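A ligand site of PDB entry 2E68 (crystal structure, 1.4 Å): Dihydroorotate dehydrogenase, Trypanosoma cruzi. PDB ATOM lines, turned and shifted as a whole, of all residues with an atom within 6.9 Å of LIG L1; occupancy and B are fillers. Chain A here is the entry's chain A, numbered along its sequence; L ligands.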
ATOM      1  N   ALA A  21      24.428   1.784  -4.021  1.00  0.00           N
ATOM      2  CA  ALA A  21      25.633   2.331  -3.393  1.00  0.00           C
ATOM      3  C   ALA A  21      25.648   3.845  -3.496  1.00  0.00           C
ATOM      4  O   ALA A  21      25.235   4.428  -4.518  1.00  0.00           O
ATOM      5  CB  ALA A  21      26.875   1.740  -4.015  1.00  0.00           C
ATOM      6  N   GLY A  22      26.083   4.482  -2.418  1.00  0.00           N
ATOM      7  CA  GLY A  22      26.151   5.936  -2.354  1.00  0.00           C
ATOM      8  C   GLY A  22      24.981   6.607  -1.681  1.00  0.00           C
ATOM      9  O   GLY A  22      25.106   7.739  -1.214  1.00  0.00           O
ATOM     10  N   LYS A  45      28.841   3.035   1.009  1.00  0.00           N
ATOM     11  CA  LYS A  45      29.327   4.042   0.052  1.00  0.00           C
ATOM     12  C   LYS A  45      30.614   3.601  -0.628  1.00  0.00           C
ATOM     13  O   LYS A  45      31.520   3.117   0.048  1.00  0.00           O
ATOM     14  CB  LYS A  45      29.566   5.367   0.806  1.00  0.00           C
ATOM     15  CG  LYS A  45      30.335   6.463   0.032  1.00  0.00           C
ATOM     16  CD  LYS A  45      29.485   7.029  -1.110  1.00  0.00           C
ATOM     17  CE  LYS A  45      30.305   7.907  -2.044  1.00  0.00           C
ATOM     18  NZ  LYS A  45      29.484   8.306  -3.243  1.00  0.00           N
ATOM     19  N   SER A  46      30.735   3.787  -1.942  1.00  0.00           N
ATOM     20  CA  SER A  46      31.992   3.475  -2.619  1.00  0.00           C
ATOM     21  C   SER A  46      33.131   4.230  -1.951  1.00  0.00           C
ATOM     22  O   SER A  46      33.067   5.465  -1.782  1.00  0.00           O
ATOM     23  CB  SER A  46      31.947   3.815  -4.104  1.00  0.00           C
ATOM     24  OG  SER A  46      31.107   2.913  -4.797  1.00  0.00           O
ATOM     25  N   ASN A  55      33.514  16.490  -4.273  1.00  0.00           N
ATOM     26  CA  ASN A  55      33.436  17.688  -5.110  1.00  0.00           C
ATOM     27  C   ASN A  55      32.720  18.847  -4.377  1.00  0.00           C
ATOM     28  O   ASN A  55      32.027  18.628  -3.398  1.00  0.00           O
ATOM     29  CB  ASN A  55      32.719  17.364  -6.429  1.00  0.00           C
ATOM     30  CG  ASN A  55      33.506  16.420  -7.332  1.00  0.00           C
ATOM     31  OD1 ASN A  55      34.729  16.260  -7.212  1.00  0.00           O
ATOM     32  ND2 ASN A  55      32.808  15.793  -8.279  1.00  0.00           N
ATOM     33  N   ASN A  69      23.872  14.197 -10.069  1.00  0.00           N
ATOM     34  CA  ASN A  69      24.832  14.265  -8.991  1.00  0.00           C
ATOM     35  C   ASN A  69      26.256  14.262  -9.503  1.00  0.00           C
ATOM     36  O   ASN A  69      26.574  13.596 -10.481  1.00  0.00           O
ATOM     37  CB  ASN A  69      24.644  13.131  -7.963  1.00  0.00           C
ATOM     38  CG  ASN A  69      25.462  11.884  -8.284  1.00  0.00           C
ATOM     39  OD1 ASN A  69      26.660  11.785  -7.960  1.00  0.00           O
ATOM     40  ND2 ASN A  69      24.818  10.882  -8.901  1.00  0.00           N
ATOM     41  N   SER A  70      27.109  15.037  -8.829  1.00  0.00           N
ATOM     42  CA  SER A  70      28.550  14.915  -9.005  1.00  0.00           C
ATOM     43  C   SER A  70      29.191  14.917  -7.631  1.00  0.00           C
ATOM     44  O   SER A  70      29.914  15.850  -7.274  1.00  0.00           O
ATOM     45  CB  SER A  70      29.096  16.034  -9.883  1.00  0.00           C
ATOM     46  OG  SER A  70      30.480  15.846 -10.142  1.00  0.00           O
ATOM     47  N   MET A  71      28.911  13.877  -6.848  1.00  0.00           N
ATOM     48  CA  MET A  71      29.376  13.821  -5.460  1.00  0.00           C
ATOM     49  C   MET A  71      30.910  13.843  -5.384  1.00  0.00           C
ATOM     50  O   MET A  71      31.476  14.565  -4.550  1.00  0.00           O
ATOM     51  CB  MET A  71      28.844  12.597  -4.710  1.00  0.00           C
ATOM     52  CG  MET A  71      27.328  12.429  -4.744  1.00  0.00           C
ATOM     53  SD  MET A  71      26.366  13.826  -4.146  1.00  0.00           S
ATOM     54  CE  MET A  71      26.705  13.730  -2.399  1.00  0.00           C
ATOM     55  N   GLY A  72      31.566  13.065  -6.231  1.00  0.00           N
ATOM     56  CA  GLY A  72      33.028  12.986  -6.273  1.00  0.00           C
ATOM     57  C   GLY A  72      33.609  12.044  -5.231  1.00  0.00           C
ATOM     58  O   GLY A  72      34.708  12.281  -4.726  1.00  0.00           O
ATOM     59  N   LEU A  73      32.877  10.962  -4.933  1.00  0.00           N
ATOM     60  CA  LEU A  73      33.301   9.940  -3.957  1.00  0.00           C
ATOM     61  C   LEU A  73      33.649  10.495  -2.556  1.00  0.00           C
ATOM     62  O   LEU A  73      34.678  10.111  -1.981  1.00  0.00           O
ATOM     63  CB  LEU A  73      34.448   9.078  -4.505  1.00  0.00           C
ATOM     64  CG  LEU A  73      34.134   8.215  -5.727  1.00  0.00           C
ATOM     65  CD1 LEU A  73      35.411   7.576  -6.272  1.00  0.00           C
ATOM     66  CD2 LEU A  73      33.079   7.137  -5.418  1.00  0.00           C
ATOM     67  N   PRO A  74      32.779  11.354  -1.990  1.00  0.00           N
ATOM     68  CA  PRO A  74      33.007  11.753  -0.601  1.00  0.00           C
ATOM     69  C   PRO A  74      32.798  10.505   0.245  1.00  0.00           C
ATOM     70  O   PRO A  74      31.791   9.812   0.099  1.00  0.00           O
ATOM     71  CB  PRO A  74      31.908  12.776  -0.322  1.00  0.00           C
ATOM     72  CG  PRO A  74      30.830  12.501  -1.328  1.00  0.00           C
ATOM     73  CD  PRO A  74      31.514  11.895  -2.533  1.00  0.00           C
ATOM     74  N   SER A 101      35.819   1.944  -4.786  1.00  0.00           N
ATOM     75  CA  SER A 101      36.026   2.679  -6.025  1.00  0.00           C
ATOM     76  C   SER A 101      37.366   3.394  -6.007  1.00  0.00           C
ATOM     77  O   SER A 101      37.423   4.619  -6.043  1.00  0.00           O
ATOM     78  CB  SER A 101      34.881   3.657  -6.266  1.00  0.00           C
ATOM     79  OG  SER A 101      34.935   4.181  -7.582  1.00  0.00           O
ATOM     80  N   ASN A 129      33.389  -1.052  -7.973  1.00  0.00           N
ATOM     81  CA  ASN A 129      32.779   0.005  -8.788  1.00  0.00           C
ATOM     82  C   ASN A 129      33.672   0.411  -9.960  1.00  0.00           C
ATOM     83  O   ASN A 129      34.705   1.055  -9.758  1.00  0.00           O
ATOM     84  CB  ASN A 129      32.475   1.216  -7.890  1.00  0.00           C
ATOM     85  CG  ASN A 129      31.774   2.340  -8.624  1.00  0.00           C
ATOM     86  OD1 ASN A 129      31.542   2.291  -9.834  1.00  0.00           O
ATOM     87  ND2 ASN A 129      31.397   3.362  -7.881  1.00  0.00           N
ATOM     88  N   SER A 131      32.521   2.281 -12.566  1.00  0.00           N
ATOM     89  CA  SER A 131      31.619   3.137 -13.325  1.00  0.00           C
ATOM     90  C   SER A 131      31.343   4.522 -12.731  1.00  0.00           C
ATOM     91  O   SER A 131      30.406   5.180 -13.151  1.00  0.00           O
ATOM     92  CB  SER A 131      30.316   2.385 -13.597  1.00  0.00           C
ATOM     93  OG  SER A 131      29.823   1.757 -12.437  1.00  0.00           O
ATOM     94  N   CYS A 132      32.162   4.969 -11.797  1.00  0.00           N
ATOM     95  CA  CYS A 132      32.007   6.328 -11.276  1.00  0.00           C
ATOM     96  C   CYS A 132      32.251   7.342 -12.396  1.00  0.00           C
ATOM     97  O   CYS A 132      33.311   7.352 -13.011  1.00  0.00           O
ATOM     98  CB  CYS A 132      32.979   6.576 -10.133  1.00  0.00           C
ATOM     99  SG  CYS A 132      32.966   8.289  -9.527  1.00  0.00           S
ATOM    100  N   PRO A 133      31.250   8.202 -12.678  1.00  0.00           N
ATOM    101  CA  PRO A 133      31.387   9.186 -13.751  1.00  0.00           C
ATOM    102  C   PRO A 133      31.684  10.623 -13.281  1.00  0.00           C
ATOM    103  O   PRO A 133      31.549  11.562 -14.075  1.00  0.00           O
ATOM    104  CB  PRO A 133      29.994   9.157 -14.369  1.00  0.00           C
ATOM    105  CG  PRO A 133      29.074   8.995 -13.151  1.00  0.00           C
ATOM    106  CD  PRO A 133      29.894   8.251 -12.091  1.00  0.00           C
ATOM    107  N   ASN A 134      32.094  10.791 -12.018  1.00  0.00           N
ATOM    108  CA  ASN A 134      32.118  12.123 -11.389  1.00  0.00           C
ATOM    109  C   ASN A 134      33.450  12.660 -10.861  1.00  0.00           C
ATOM    110  O   ASN A 134      33.506  13.786 -10.361  1.00  0.00           O
ATOM    111  CB  ASN A 134      31.079  12.192 -10.260  1.00  0.00           C
ATOM    112  CG  ASN A 134      29.660  12.037 -10.766  1.00  0.00           C
ATOM    113  OD1 ASN A 134      29.324  12.481 -11.867  1.00  0.00           O
ATOM    114  ND2 ASN A 134      28.819  11.415  -9.958  1.00  0.00           N
ATOM    115  N   VAL A 135      34.521  11.870 -10.938  1.00  0.00           N
ATOM    116  CA  VAL A 135      35.820  12.365 -10.456  1.00  0.00           C
ATOM    117  C   VAL A 135      36.537  13.033 -11.633  1.00  0.00           C
ATOM    118  O   VAL A 135      36.768  12.385 -12.649  1.00  0.00           O
ATOM    119  CB  VAL A 135      36.665  11.254  -9.805  1.00  0.00           C
ATOM    120  CG1 VAL A 135      38.060  11.785  -9.433  1.00  0.00           C
ATOM    121  CG2 VAL A 135      35.957  10.716  -8.583  1.00  0.00           C
ATOM    122  N   LYS A 166      29.999  -3.162 -10.326  1.00  0.00           N
ATOM    123  CA  LYS A 166      29.023  -2.115 -10.637  1.00  0.00           C
ATOM    124  C   LYS A 166      29.374  -1.554 -12.014  1.00  0.00           C
ATOM    125  O   LYS A 166      30.434  -0.927 -12.195  1.00  0.00           O
ATOM    126  CB  LYS A 166      29.050  -1.020  -9.561  1.00  0.00           C
ATOM    127  CG  LYS A 166      28.036   0.104  -9.750  1.00  0.00           C
ATOM    128  CD  LYS A 166      26.598  -0.351  -9.538  1.00  0.00           C
ATOM    129  CE  LYS A 166      25.606   0.821  -9.450  1.00  0.00           C
ATOM    130  NZ  LYS A 166      25.756   1.602  -8.192  1.00  0.00           N
ATOM    131  N   ASN A 196      25.077   1.887 -12.906  1.00  0.00           N
ATOM    132  CA  ASN A 196      25.446   3.160 -12.294  1.00  0.00           C
ATOM    133  C   ASN A 196      24.715   4.310 -13.013  1.00  0.00           C
ATOM    134  O   ASN A 196      23.990   4.077 -13.997  1.00  0.00           O
ATOM    135  CB  ASN A 196      26.978   3.326 -12.363  1.00  0.00           C
ATOM    136  CG  ASN A 196      27.546   4.144 -11.203  1.00  0.00           C
ATOM    137  OD1 ASN A 196      27.023   5.209 -10.853  1.00  0.00           O
ATOM    138  ND2 ASN A 196      28.625   3.651 -10.602  1.00  0.00           N
ATOM    139  N   SER A 197      24.896   5.539 -12.523  1.00  0.00           N
ATOM    140  CA  SER A 197      24.210   6.685 -13.121  1.00  0.00           C
ATOM    141  C   SER A 197      24.601   6.870 -14.589  1.00  0.00           C
ATOM    142  O   SER A 197      25.681   6.456 -15.036  1.00  0.00           O
ATOM    143  CB  SER A 197      24.502   7.960 -12.326  1.00  0.00           C
ATOM    144  OG  SER A 197      25.892   8.237 -12.312  1.00  0.00           O
ATOM    145  N   VAL A 198      23.678   7.457 -15.348  1.00  0.00           N
ATOM    146  CA  VAL A 198      23.928   7.756 -16.762  1.00  0.00           C
ATOM    147  C   VAL A 198      24.818   9.002 -16.807  1.00  0.00           C
ATOM    148  O   VAL A 198      24.405  10.111 -16.447  1.00  0.00           O
ATOM    149  CB  VAL A 198      22.590   7.914 -17.508  1.00  0.00           C
ATOM    150  CG1 VAL A 198      22.811   8.477 -18.900  1.00  0.00           C
ATOM    151  CG2 VAL A 198      21.875   6.564 -17.585  1.00  0.00           C
ATOM    152  N   GLY A 220      26.890  15.985 -14.556  1.00  0.00           N
ATOM    153  CA  GLY A 220      26.765  14.982 -13.491  1.00  0.00           C
ATOM    154  C   GLY A 220      25.966  13.784 -13.937  1.00  0.00           C
ATOM    155  O   GLY A 220      25.300  13.814 -14.994  1.00  0.00           O
ATOM    156  N   GLY A 221      26.024  12.722 -13.137  1.00  0.00           N
ATOM    157  CA  GLY A 221      25.357  11.476 -13.459  1.00  0.00           C
ATOM    158  C   GLY A 221      23.863  11.538 -13.185  1.00  0.00           C
ATOM    159  O   GLY A 221      23.433  12.108 -12.168  1.00  0.00           O
ATOM    160  N   LEU A 222      23.078  10.973 -14.091  1.00  0.00           N
ATOM    161  CA  LEU A 222      21.618  10.988 -13.981  1.00  0.00           C
ATOM    162  C   LEU A 222      21.085   9.711 -13.359  1.00  0.00           C
ATOM    163  O   LEU A 222      21.537   8.603 -13.676  1.00  0.00           O
ATOM    164  CB  LEU A 222      20.970  11.182 -15.358  1.00  0.00           C
ATOM    165  CG  LEU A 222      21.440  12.393 -16.168  1.00  0.00           C
ATOM    166  CD1 LEU A 222      20.885  12.329 -17.583  1.00  0.00           C
ATOM    167  CD2 LEU A 222      21.080  13.719 -15.497  1.00  0.00           C
HETATM  168  O1  LIG L   1      26.529   8.521  -9.624  1.00  0.00           O
HETATM  169  C1  LIG L   1      27.543   8.249  -8.964  1.00  0.00           C
HETATM  170  N1  LIG L   1      28.034   9.128  -8.092  1.00  0.00           N
HETATM  171  N2  LIG L   1      28.155   7.071  -9.148  1.00  0.00           N
HETATM  172  C2  LIG L   1      29.318   6.717  -8.582  1.00  0.00           C
HETATM  173  O2  LIG L   1      29.819   5.615  -8.746  1.00  0.00           O
HETATM  174  C3  LIG L   1      30.015   7.708  -7.696  1.00  0.00           C
HETATM  175  C4  LIG L   1      29.071   8.752  -7.123  1.00  0.00           C
HETATM  176  C5  LIG L   1      29.915   9.898  -6.657  1.00  0.00           C
HETATM  177  O3  LIG L   1      30.043  10.903  -7.390  1.00  0.00           O
HETATM  178  O4  LIG L   1      30.459   9.771  -5.529  1.00  0.00           O
HETATM  179  N1  LG2 L   2      27.013   4.353  -7.263  1.00  0.00           N
HETATM  180  C1  LG2 L   2      28.132   3.673  -6.849  1.00  0.00           C
HETATM  181  O1  LG2 L   2      28.426   2.596  -7.370  1.00  0.00           O
HETATM  182  N2  LG2 L   2      28.896   4.187  -5.829  1.00  0.00           N
HETATM  183  C2  LG2 L   2      28.607   5.379  -5.197  1.00  0.00           C
HETATM  184  O2  LG2 L   2      29.225   5.697  -4.161  1.00  0.00           O
HETATM  185  C3  LG2 L   2      27.466   6.060  -5.612  1.00  0.00           C
HETATM  186  N3  LG2 L   2      27.094   7.255  -5.024  1.00  0.00           N
HETATM  187  C4  LG2 L   2      25.926   7.889  -5.405  1.00  0.00           C
HETATM  188  C5  LG2 L   2      25.550   9.092  -4.806  1.00  0.00           C
HETATM  189  C6  LG2 L   2      24.375   9.754  -5.201  1.00  0.00           C
HETATM  190  C7  LG2 L   2      23.833  10.806  -4.266  1.00  0.00           C
HETATM  191  C8  LG2 L   2      23.595   9.202  -6.226  1.00  0.00           C
HETATM  192  C9  LG2 L   2      22.186   9.688  -6.468  1.00  0.00           C
HETATM  193  C10 LG2 L   2      23.995   8.013  -6.836  1.00  0.00           C
HETATM  194  C11 LG2 L   2      25.152   7.358  -6.434  1.00  0.00           C
HETATM  195  N4  LG2 L   2      25.549   6.181  -7.063  1.00  0.00           N
HETATM  196  C12 LG2 L   2      26.679   5.528  -6.645  1.00  0.00           C
HETATM  197  C13 LG2 L   2      24.823   5.674  -8.259  1.00  0.00           C
HETATM  198  C14 LG2 L   2      23.675   4.802  -7.742  1.00  0.00           C
HETATM  199  O3  LG2 L   2      24.180   3.699  -7.007  1.00  0.00           O
HETATM  200  C15 LG2 L   2      22.769   4.276  -8.853  1.00  0.00           C
HETATM  201  O4  LG2 L   2      23.561   3.426  -9.659  1.00  0.00           O
HETATM  202  C16 LG2 L   2      22.150   5.380  -9.708  1.00  0.00           C
HETATM  203  O5  LG2 L   2      21.773   6.478  -8.892  1.00  0.00           O
HETATM  204  C17 LG2 L   2      20.960   4.881 -10.524  1.00  0.00           C
HETATM  205  O6  LG2 L   2      19.923   4.409  -9.691  1.00  0.00           O
HETATM  206  P1  LG2 L   2      18.602   5.293  -9.412  1.00  0.00           P
HETATM  207  O7  LG2 L   2      17.932   5.561 -10.741  1.00  0.00           O
HETATM  208  O8  LG2 L   2      17.777   4.481  -8.437  1.00  0.00           O
HETATM  209  O9  LG2 L   2      19.073   6.601  -8.805  1.00  0.00           O
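OD1 of Asn 129 lies within hydrogen-bond range of ND2 of Asn 196 (3.3 Å).
The side-chain amide nitrogen (ND2) of Asn 196 is in hydrogen-bond range of the side-chain hydroxyl (OG) of Ser 131 (2.9 Å).
OD1 of Asn 129 lies within hydrogen-bond range of N of Cys 132 (3.4 Å).
The side-chain amide nitrogen (ND2) of Asn 129 sits at hydrogen-bond distance from the side-chain hydroxyl (OG) of Ser 46 (3.1 Å).
O of Asn 134 sits at hydrogen-bond distance from ND2 of Asn 55 (3.0 Å).
N of Met 71 is in hydrogen-bond range of OD1 of Asn 69 (3.3 Å).
The backbone carbonyl oxygen of Asn 69 lies within hydrogen-bond range of the backbone NH of Gly 221.
The backbone NH of Asn 55 lies within hydrogen-bond range of the backbone carbonyl oxygen of Met 71 (2.8 Å).
An oxygen (O4) of LIG L1 lies within hydrogen-bond range of the backbone NH (N) of Leu 73 (2.8 Å).
The side-chain amide oxygen (OD1) of Asn 196 lies within hydrogen-bond range of a nitrogen (N2) of LIG L1, 2.8 Å away.
An oxygen (O1) of LIG L1 sits at hydrogen-bond distance from the side-chain hydroxyl (OG) of Ser 197.
An oxygen (O2) of LIG L1 is in hydrogen-bond range of the side-chain amide nitrogen (ND2) of Asn 129, at 2.9 Å.
An oxygen (O4) of LIG L1 lies within salt-bridge range of the side-chain amino group of Lys 45 (2.9 Å).
N of Gly 72 sits at hydrogen-bond distance from O3 of LIG L1, 2.9 Å away.
ND2 of Asn 134 is in hydrogen-bond range of O3 of LIG L1, at 2.9 Å.
The side-chain amide oxygen (OD1) of Asn 69 is in hydrogen-bond range of a nitrogen (N1) of LIG L1, at 3.0 Å.
N of Met 71 lies within hydrogen-bond range of O3 of LIG L1 (3.2 Å).
The side-chain amide nitrogen (ND2) of Asn 196 sits at hydrogen-bond distance from an oxygen (O1) of LG2 L2 (3.4 Å).
An oxygen (O1) of LG2 L2 is in hydrogen-bond range of the side-chain amide nitrogen (ND2) of Asn 129, 3.1 Å away.
The side-chain amino group (NZ) of Lys 45 sits at hydrogen-bond distance from an oxygen (O2) of LG2 L2, 2.8 Å away.
The backbone NH (N) of Ser 46 sits at hydrogen-bond distance from an oxygen (O2) of LG2 L2, 3.3 Å away.
OG of Ser 46 is in hydrogen-bond range of N2 of LG2 L2 (2.8 Å).
NZ of Lys 166 is in hydrogen-bond range of O3 of LG2 L2, 2.9 Å away.
O3 of LG2 L2 lies close to O of Ala 21 (2.8 Å).
Pro 74 touches LIG L1.
CA of Cys 132 touches O2 of LIG L1, at 3.4 Å.
Pro 133 touches LIG L1 (CD to N2, 3.6 Å).
Within 4 Å of LIG L1: Lys 45, Asn 69, Met 71, Gly 72, Leu 73, Pro 74, Asn 129, Cys 132, Pro 133, Asn 134, Asn 196 and Ser 197.
An oxygen (O2) of LIG L1 sits close to a nitrogen (N2) of LG2 L2.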
